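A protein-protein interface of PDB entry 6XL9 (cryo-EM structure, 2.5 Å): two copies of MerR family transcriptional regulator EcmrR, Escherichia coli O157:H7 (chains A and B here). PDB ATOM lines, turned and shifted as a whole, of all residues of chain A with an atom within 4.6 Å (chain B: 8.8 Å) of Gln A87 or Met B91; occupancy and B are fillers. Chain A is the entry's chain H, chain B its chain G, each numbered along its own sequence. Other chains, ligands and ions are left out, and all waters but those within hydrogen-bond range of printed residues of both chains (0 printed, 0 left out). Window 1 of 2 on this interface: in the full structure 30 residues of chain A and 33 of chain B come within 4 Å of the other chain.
Of the 17 printed residues of chain B, 4 touch a printed residue of chain A.
Hydrophobic or aromatic side chains of chain B within 4 Å of the printed part of chain A: Ile B84, Ile B88, Met B91 and Leu B95.
Among the printed residues, no Asp or Glu carboxylate lies within 4 Å of a Lys or Arg side-chain nitrogen of the other chain.
NE2 of Gln A87 is in hydrogen-bond range of OE2 of Glu A83, at 3.2 Å.
The side-chain amide oxygen of Gln A87 sits close to the side-chain carboxylate of Asp A90.
Met B91 touches Ile A84.
Ile A84 touches Leu B95 (CD1 to CB, 3.7 Å).
CB of Gln A87 touches CE of Met B91, at 3.7 Å.
Ile B88 touches Ile A88 (CD1 to CG1, 3.5 Å).
Ile A88 touches Leu B95 (CD1 to CD2, 3.6 Å).
Met A91 touches Ile B84 (CB to CD1, 3.5 Å).
Of chain B, only Met B91 (3.7 Å) comes within 4 Å of Gln A87.
Of chain A, only Ile A84 (3.6 Å) and Gln A87 (3.7 Å) come within 4 Å of Met B91.
Printed residues of chain A within 4 Å of Leu B95: Ile A84 and Ile A88.
Of the printed residues of chain A, Ile B88 touches Ile A88.
Of the printed residues of chain B, Ile A84 touches Met B91 (3.6 Å) and Leu B95 (3.7 Å).
Asp B90 touches none of the printed residues of chain A.
The nearest residue of chain B that does not touch Gln A87 is Ile B88 (5.3 Å).
The nearest printed residue of chain B that does not touch Ile A88 is Met B91 (4.7 Å).
Ile A84 touches Met B91, and with the chains exchanged Met A91 touches Ile B84.
Gln A87 touches Met B91, but with the chains exchanged Met A91 does not touch Gln B87 (5.3 Å).
Ile A88 touches its own counterpart, Ile B88.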
ATOM      1  N   ARG A  80      30.372  10.367  19.251  1.00  0.00           N
ATOM      2  CA  ARG A  80      29.305  11.087  19.924  1.00  0.00           C
ATOM      3  C   ARG A  80      28.114  10.157  20.139  1.00  0.00           C
ATOM      4  O   ARG A  80      27.382  10.310  21.126  1.00  0.00           O
ATOM      5  CB  ARG A  80      28.909  12.298  19.080  1.00  0.00           C
ATOM      6  CG  ARG A  80      27.730  13.110  19.567  1.00  0.00           C
ATOM      7  CD  ARG A  80      28.090  14.035  20.706  1.00  0.00           C
ATOM      8  NE  ARG A  80      26.907  14.752  21.177  1.00  0.00           N
ATOM      9  CZ  ARG A  80      26.615  14.977  22.452  1.00  0.00           C
ATOM     10  NH1 ARG A  80      25.515  15.641  22.768  1.00  0.00           N
ATOM     11  NH2 ARG A  80      27.432  14.561  23.402  1.00  0.00           N
ATOM     12  N   GLU A  83      28.558   8.321  23.430  1.00  0.00           N
ATOM     13  CA  GLU A  83      28.380   9.177  24.598  1.00  0.00           C
ATOM     14  C   GLU A  83      26.921   9.563  24.806  1.00  0.00           C
ATOM     15  O   GLU A  83      26.492   9.729  25.952  1.00  0.00           O
ATOM     16  CB  GLU A  83      29.252  10.429  24.472  1.00  0.00           C
ATOM     17  CG  GLU A  83      29.207  11.388  25.666  1.00  0.00           C
ATOM     18  CD  GLU A  83      28.025  12.339  25.618  1.00  0.00           C
ATOM     19  OE1 GLU A  83      27.528  12.606  24.503  1.00  0.00           O
ATOM     20  OE2 GLU A  83      27.587  12.805  26.688  1.00  0.00           O
ATOM     21  N   ILE A  84      26.150   9.730  23.727  1.00  0.00           N
ATOM     22  CA  ILE A  84      24.727  10.018  23.902  1.00  0.00           C
ATOM     23  C   ILE A  84      24.037   8.871  24.630  1.00  0.00           C
ATOM     24  O   ILE A  84      23.201   9.102  25.506  1.00  0.00           O
ATOM     25  CB  ILE A  84      24.027  10.426  22.589  1.00  0.00           C
ATOM     26  CG1 ILE A  84      24.045   9.354  21.519  1.00  0.00           C
ATOM     27  CG2 ILE A  84      24.637  11.722  22.056  1.00  0.00           C
ATOM     28  CD1 ILE A  84      23.521   9.874  20.198  1.00  0.00           C
ATOM     29  N   GLN A  85      24.322   7.621  24.246  1.00  0.00           N
ATOM     30  CA  GLN A  85      23.678   6.499  24.926  1.00  0.00           C
ATOM     31  C   GLN A  85      24.125   6.430  26.381  1.00  0.00           C
ATOM     32  O   GLN A  85      23.329   6.099  27.272  1.00  0.00           O
ATOM     33  CB  GLN A  85      23.990   5.179  24.221  1.00  0.00           C
ATOM     34  CG  GLN A  85      23.818   5.185  22.719  1.00  0.00           C
ATOM     35  CD  GLN A  85      22.367   5.230  22.289  1.00  0.00           C
ATOM     36  OE1 GLN A  85      21.959   6.101  21.522  1.00  0.00           O
ATOM     37  NE2 GLN A  85      21.579   4.288  22.784  1.00  0.00           N
ATOM     38  N   LYS A  86      25.400   6.713  26.643  1.00  0.00           N
ATOM     39  CA  LYS A  86      25.838   6.754  28.034  1.00  0.00           C
ATOM     40  C   LYS A  86      25.069   7.811  28.817  1.00  0.00           C
ATOM     41  O   LYS A  86      24.636   7.568  29.952  1.00  0.00           O
ATOM     42  CB  LYS A  86      27.333   7.034  28.118  1.00  0.00           C
ATOM     43  CG  LYS A  86      27.831   7.085  29.549  1.00  0.00           C
ATOM     44  CD  LYS A  86      27.661   5.752  30.247  1.00  0.00           C
ATOM     45  CE  LYS A  86      28.262   5.779  31.644  1.00  0.00           C
ATOM     46  NZ  LYS A  86      27.511   6.704  32.543  1.00  0.00           N
ATOM     47  N   GLN A  87      24.912   8.998  28.230  1.00  0.00           N
ATOM     48  CA  GLN A  87      24.169  10.069  28.880  1.00  0.00           C
ATOM     49  C   GLN A  87      22.698   9.713  29.063  1.00  0.00           C
ATOM     50  O   GLN A  87      22.086  10.062  30.076  1.00  0.00           O
ATOM     51  CB  GLN A  87      24.305  11.355  28.066  1.00  0.00           C
ATOM     52  CG  GLN A  87      23.925  12.620  28.814  1.00  0.00           C
ATOM     53  CD  GLN A  87      24.962  13.020  29.840  1.00  0.00           C
ATOM     54  OE1 GLN A  87      24.796  12.776  31.034  1.00  0.00           O
ATOM     55  NE2 GLN A  87      26.040  13.643  29.378  1.00  0.00           N
ATOM     56  N   ILE A  88      22.092   9.038  28.091  1.00  0.00           N
ATOM     57  CA  ILE A  88      20.698   8.662  28.291  1.00  0.00           C
ATOM     58  C   ILE A  88      20.571   7.689  29.459  1.00  0.00           C
ATOM     59  O   ILE A  88      19.694   7.848  30.314  1.00  0.00           O
ATOM     60  CB  ILE A  88      20.052   8.148  26.980  1.00  0.00           C
ATOM     61  CG1 ILE A  88      18.537   8.142  27.109  1.00  0.00           C
ATOM     62  CG2 ILE A  88      20.472   6.758  26.586  1.00  0.00           C
ATOM     63  CD1 ILE A  88      17.829   7.853  25.810  1.00  0.00           C
ATOM     64  N   ARG A  89      21.439   6.669  29.520  1.00  0.00           N
ATOM     65  CA  ARG A  89      21.357   5.722  30.630  1.00  0.00           C
ATOM     66  C   ARG A  89      21.684   6.336  31.991  1.00  0.00           C
ATOM     67  O   ARG A  89      20.996   6.038  32.979  1.00  0.00           O
ATOM     68  CB  ARG A  89      22.281   4.536  30.364  1.00  0.00           C
ATOM     69  CG  ARG A  89      21.737   3.576  29.329  1.00  0.00           C
ATOM     70  CD  ARG A  89      22.383   2.223  29.452  1.00  0.00           C
ATOM     71  NE  ARG A  89      23.836   2.317  29.405  1.00  0.00           N
ATOM     72  CZ  ARG A  89      24.551   2.255  28.287  1.00  0.00           C
ATOM     73  NH1 ARG A  89      23.939   2.102  27.119  1.00  0.00           N
ATOM     74  NH2 ARG A  89      25.871   2.343  28.330  1.00  0.00           N
ATOM     75  N   ASP A  90      22.631   7.282  32.057  1.00  0.00           N
ATOM     76  CA  ASP A  90      22.913   7.879  33.363  1.00  0.00           C
ATOM     77  C   ASP A  90      21.773   8.789  33.794  1.00  0.00           C
ATOM     78  O   ASP A  90      21.410   8.804  34.974  1.00  0.00           O
ATOM     79  CB  ASP A  90      24.311   8.530  33.425  1.00  0.00           C
ATOM     80  CG  ASP A  90      24.413   9.898  32.786  1.00  0.00           C
ATOM     81  OD1 ASP A  90      23.536  10.313  32.040  1.00  0.00           O
ATOM     82  OD2 ASP A  90      25.406  10.596  33.073  1.00  0.00           O
ATOM     83  N   MET A  91      21.229   9.598  32.875  1.00  0.00           N
ATOM     84  CA  MET A  91      20.122  10.457  33.276  1.00  0.00           C
ATOM     85  C   MET A  91      18.907   9.615  33.648  1.00  0.00           C
ATOM     86  O   MET A  91      18.196   9.934  34.610  1.00  0.00           O
ATOM     87  CB  MET A  91      19.786  11.432  32.150  1.00  0.00           C
ATOM     88  CG  MET A  91      20.892  12.408  31.735  1.00  0.00           C
ATOM     89  SD  MET A  91      21.429  13.612  32.982  1.00  0.00           S
ATOM     90  CE  MET A  91      22.803  12.816  33.805  1.00  0.00           C
ATOM     91  N   ARG B  80      14.291  19.589  40.668  1.00  0.00           N
ATOM     92  CA  ARG B  80      15.350  18.915  39.926  1.00  0.00           C
ATOM     93  C   ARG B  80      14.755  17.827  39.056  1.00  0.00           C
ATOM     94  O   ARG B  80      15.235  17.579  37.944  1.00  0.00           O
ATOM     95  CB  ARG B  80      16.378  18.339  40.902  1.00  0.00           C
ATOM     96  CG  ARG B  80      17.390  17.366  40.307  1.00  0.00           C
ATOM     97  CD  ARG B  80      18.560  18.056  39.621  1.00  0.00           C
ATOM     98  NE  ARG B  80      19.343  17.098  38.845  1.00  0.00           N
ATOM     99  CZ  ARG B  80      20.022  17.391  37.744  1.00  0.00           C
ATOM    100  NH1 ARG B  80      20.024  18.631  37.274  1.00  0.00           N
ATOM    101  NH2 ARG B  80      20.702  16.443  37.112  1.00  0.00           N
ATOM    102  N   ILE B  84      15.556  16.996  35.057  1.00  0.00           N
ATOM    103  CA  ILE B  84      15.940  15.738  34.436  1.00  0.00           C
ATOM    104  C   ILE B  84      14.880  15.296  33.431  1.00  0.00           C
ATOM    105  O   ILE B  84      15.217  14.878  32.317  1.00  0.00           O
ATOM    106  CB  ILE B  84      16.228  14.672  35.516  1.00  0.00           C
ATOM    107  CG1 ILE B  84      16.805  13.410  34.888  1.00  0.00           C
ATOM    108  CG2 ILE B  84      15.033  14.374  36.380  1.00  0.00           C
ATOM    109  CD1 ILE B  84      18.168  13.621  34.358  1.00  0.00           C
ATOM    110  N   GLN B  85      13.594  15.373  33.804  1.00  0.00           N
ATOM    111  CA  GLN B  85      12.541  14.885  32.915  1.00  0.00           C
ATOM    112  C   GLN B  85      12.586  15.647  31.598  1.00  0.00           C
ATOM    113  O   GLN B  85      12.364  15.073  30.529  1.00  0.00           O
ATOM    114  CB  GLN B  85      11.153  14.943  33.569  1.00  0.00           C
ATOM    115  CG  GLN B  85      10.491  16.294  33.706  1.00  0.00           C
ATOM    116  CD  GLN B  85       9.649  16.672  32.511  1.00  0.00           C
ATOM    117  OE1 GLN B  85       9.627  15.981  31.486  1.00  0.00           O
ATOM    118  NE2 GLN B  85       8.936  17.785  32.618  1.00  0.00           N
ATOM    119  N   LYS B  86      12.806  16.960  31.671  1.00  0.00           N
ATOM    120  CA  LYS B  86      13.005  17.746  30.463  1.00  0.00           C
ATOM    121  C   LYS B  86      14.242  17.258  29.718  1.00  0.00           C
ATOM    122  O   LYS B  86      14.181  16.984  28.513  1.00  0.00           O
ATOM    123  CB  LYS B  86      13.140  19.227  30.829  1.00  0.00           C
ATOM    124  CG  LYS B  86      14.041  20.044  29.911  1.00  0.00           C
ATOM    125  CD  LYS B  86      13.648  21.507  29.889  1.00  0.00           C
ATOM    126  CE  LYS B  86      13.781  22.093  31.288  1.00  0.00           C
ATOM    127  NZ  LYS B  86      13.449  23.542  31.365  1.00  0.00           N
ATOM    128  N   GLN B  87      15.365  17.095  30.435  1.00  0.00           N
ATOM    129  CA  GLN B  87      16.639  16.853  29.762  1.00  0.00           C
ATOM    130  C   GLN B  87      16.600  15.573  28.946  1.00  0.00           C
ATOM    131  O   GLN B  87      17.040  15.558  27.789  1.00  0.00           O
ATOM    132  CB  GLN B  87      17.786  16.777  30.775  1.00  0.00           C
ATOM    133  CG  GLN B  87      18.505  18.082  31.066  1.00  0.00           C
ATOM    134  CD  GLN B  87      19.706  18.302  30.167  1.00  0.00           C
ATOM    135  OE1 GLN B  87      20.185  17.378  29.506  1.00  0.00           O
ATOM    136  NE2 GLN B  87      20.199  19.534  30.136  1.00  0.00           N
ATOM    137  N   ILE B  88      16.045  14.498  29.523  1.00  0.00           N
ATOM    138  CA  ILE B  88      15.897  13.246  28.784  1.00  0.00           C
ATOM    139  C   ILE B  88      15.215  13.513  27.446  1.00  0.00           C
ATOM    140  O   ILE B  88      15.712  13.108  26.385  1.00  0.00           O
ATOM    141  CB  ILE B  88      15.192  12.175  29.646  1.00  0.00           C
ATOM    142  CG1 ILE B  88      15.439  10.792  29.064  1.00  0.00           C
ATOM    143  CG2 ILE B  88      13.707  12.400  29.859  1.00  0.00           C
ATOM    144  CD1 ILE B  88      16.866  10.385  29.192  1.00  0.00           C
ATOM    145  N   ARG B  89      14.082  14.232  27.478  1.00  0.00           N
ATOM    146  CA  ARG B  89      13.346  14.544  26.259  1.00  0.00           C
ATOM    147  C   ARG B  89      14.266  15.211  25.254  1.00  0.00           C
ATOM    148  O   ARG B  89      14.360  14.786  24.096  1.00  0.00           O
ATOM    149  CB  ARG B  89      12.171  15.453  26.612  1.00  0.00           C
ATOM    150  CG  ARG B  89      11.052  14.751  27.361  1.00  0.00           C
ATOM    151  CD  ARG B  89       9.868  15.677  27.605  1.00  0.00           C
ATOM    152  NE  ARG B  89      10.266  16.854  28.377  1.00  0.00           N
ATOM    153  CZ  ARG B  89       9.435  17.815  28.775  1.00  0.00           C
ATOM    154  NH1 ARG B  89       9.890  18.848  29.472  1.00  0.00           N
ATOM    155  NH2 ARG B  89       8.147  17.746  28.473  1.00  0.00           N
ATOM    156  N   ASP B  90      15.018  16.214  25.720  1.00  0.00           N
ATOM    157  CA  ASP B  90      15.956  16.911  24.852  1.00  0.00           C
ATOM    158  C   ASP B  90      16.949  15.924  24.270  1.00  0.00           C
ATOM    159  O   ASP B  90      17.128  15.836  23.052  1.00  0.00           O
ATOM    160  CB  ASP B  90      16.686  18.012  25.620  1.00  0.00           C
ATOM    161  CG  ASP B  90      15.742  18.995  26.274  1.00  0.00           C
ATOM    162  OD1 ASP B  90      14.985  19.678  25.556  1.00  0.00           O
ATOM    163  OD2 ASP B  90      15.775  19.098  27.515  1.00  0.00           O
ATOM    164  N   MET B  91      17.517  15.091  25.138  1.00  0.00           N
ATOM    165  CA  MET B  91      18.440  14.070  24.681  1.00  0.00           C
ATOM    166  C   MET B  91      17.749  13.140  23.699  1.00  0.00           C
ATOM    167  O   MET B  91      18.266  12.867  22.606  1.00  0.00           O
ATOM    168  CB  MET B  91      18.986  13.297  25.882  1.00  0.00           C
ATOM    169  CG  MET B  91      20.313  12.628  25.604  1.00  0.00           C
ATOM    170  SD  MET B  91      21.534  13.934  25.381  1.00  0.00           S
ATOM    171  CE  MET B  91      22.995  12.987  25.028  1.00  0.00           C
ATOM    172  N   ALA B  92      16.519  12.740  24.029  1.00  0.00           N
ATOM    173  CA  ALA B  92      15.766  11.838  23.176  1.00  0.00           C
ATOM    174  C   ALA B  92      15.471  12.416  21.801  1.00  0.00           C
ATOM    175  O   ALA B  92      15.157  11.653  20.883  1.00  0.00           O
ATOM    176  CB  ALA B  92      14.461  11.445  23.863  1.00  0.00           C
ATOM    177  N   ASP B  93      15.505  13.731  21.623  1.00  0.00           N
ATOM    178  CA  ASP B  93      15.397  14.196  20.245  1.00  0.00           C
ATOM    179  C   ASP B  93      16.721  14.011  19.498  1.00  0.00           C
ATOM    180  O   ASP B  93      16.744  13.448  18.396  1.00  0.00           O
ATOM    181  CB  ASP B  93      14.798  15.618  20.152  1.00  0.00           C
ATOM    182  CG  ASP B  93      15.742  16.745  20.535  1.00  0.00           C
ATOM    183  OD1 ASP B  93      16.958  16.566  20.591  1.00  0.00           O
ATOM    184  OD2 ASP B  93      15.230  17.854  20.796  1.00  0.00           O
ATOM    185  N   MET B  94      17.847  14.424  20.104  1.00  0.00           N
ATOM    186  CA  MET B  94      19.111  14.464  19.359  1.00  0.00           C
ATOM    187  C   MET B  94      19.602  13.091  18.911  1.00  0.00           C
ATOM    188  O   MET B  94      20.050  12.954  17.769  1.00  0.00           O
ATOM    189  CB  MET B  94      20.215  15.085  20.225  1.00  0.00           C
ATOM    190  CG  MET B  94      19.938  16.408  20.908  1.00  0.00           C
ATOM    191  SD  MET B  94      21.442  17.195  21.523  1.00  0.00           S
ATOM    192  CE  MET B  94      20.774  18.630  22.364  1.00  0.00           C
ATOM    193  N   LEU B  95      19.493  12.059  19.757  1.00  0.00           N
ATOM    194  CA  LEU B  95      19.894  10.728  19.301  1.00  0.00           C
ATOM    195  C   LEU B  95      19.086  10.294  18.085  1.00  0.00           C
ATOM    196  O   LEU B  95      19.572   9.519  17.253  1.00  0.00           O
ATOM    197  CB  LEU B  95      19.797   9.671  20.405  1.00  0.00           C
ATOM    198  CG  LEU B  95      18.457   9.336  21.054  1.00  0.00           C
ATOM    199  CD1 LEU B  95      17.650   8.392  20.170  1.00  0.00           C
ATOM    200  CD2 LEU B  95      18.653   8.726  22.382  1.00  0.00           C
ATOM    201  N   SER B  96      17.850  10.779  17.970  1.00  0.00           N
ATOM    202  CA  SER B  96      17.070  10.524  16.769  1.00  0.00           C
ATOM    203  C   SER B  96      17.640  11.301  15.595  1.00  0.00           C
ATOM    204  O   SER B  96      17.909  10.730  14.531  1.00  0.00           O
ATOM    205  CB  SER B  96      15.604  10.899  16.997  1.00  0.00           C
ATOM    206  OG  SER B  96      15.011  10.067  17.978  1.00  0.00           O
ATOM    207  N   ARG B  97      17.869  12.602  15.790  1.00  0.00           N
ATOM    208  CA  ARG B  97      18.204  13.473  14.670  1.00  0.00           C
ATOM    209  C   ARG B  97      19.539  13.086  14.052  1.00  0.00           C
ATOM    210  O   ARG B  97      19.666  13.025  12.825  1.00  0.00           O
ATOM    211  CB  ARG B  97      18.225  14.929  15.138  1.00  0.00           C
ATOM    212  CG  ARG B  97      16.852  15.472  15.493  1.00  0.00           C
ATOM    213  CD  ARG B  97      16.959  16.791  16.240  1.00  0.00           C
ATOM    214  NE  ARG B  97      17.493  17.846  15.384  1.00  0.00           N
ATOM    215  CZ  ARG B  97      17.520  19.133  15.710  1.00  0.00           C
ATOM    216  NH1 ARG B  97      17.040  19.533  16.878  1.00  0.00           N
ATOM    217  NH2 ARG B  97      18.020  20.023  14.864  1.00  0.00           N
ATOM    218  N   ILE B  98      20.537  12.795  14.887  1.00  0.00           N
ATOM    219  CA  ILE B  98      21.824  12.353  14.368  1.00  0.00           C
ATOM    220  C   ILE B  98      21.658  11.039  13.615  1.00  0.00           C
ATOM    221  O   ILE B  98      22.315  10.806  12.590  1.00  0.00           O
ATOM    222  CB  ILE B  98      22.838  12.262  15.527  1.00  0.00           C
ATOM    223  CG1 ILE B  98      24.240  11.946  15.026  1.00  0.00           C
ATOM    224  CG2 ILE B  98      22.414  11.232  16.557  1.00  0.00           C
ATOM    225  CD1 ILE B  98      25.285  12.171  16.093  1.00  0.00           C
ATOM    226  N   LYS B 267       6.442  20.275  18.240  1.00  0.00           N
ATOM    227  CA  LYS B 267       6.944  19.051  18.844  1.00  0.00           C
ATOM    228  C   LYS B 267       5.749  18.206  19.267  1.00  0.00           C
ATOM    229  O   LYS B 267       5.009  18.568  20.186  1.00  0.00           O
ATOM    230  CB  LYS B 267       7.844  19.384  20.032  1.00  0.00           C
ATOM    231  CG  LYS B 267       8.490  18.186  20.701  1.00  0.00           C
ATOM    232  CD  LYS B 267       9.291  17.358  19.715  1.00  0.00           C
ATOM    233  CE  LYS B 267      10.307  16.497  20.436  1.00  0.00           C
ATOM    234  NZ  LYS B 267       9.642  15.488  21.299  1.00  0.00           N
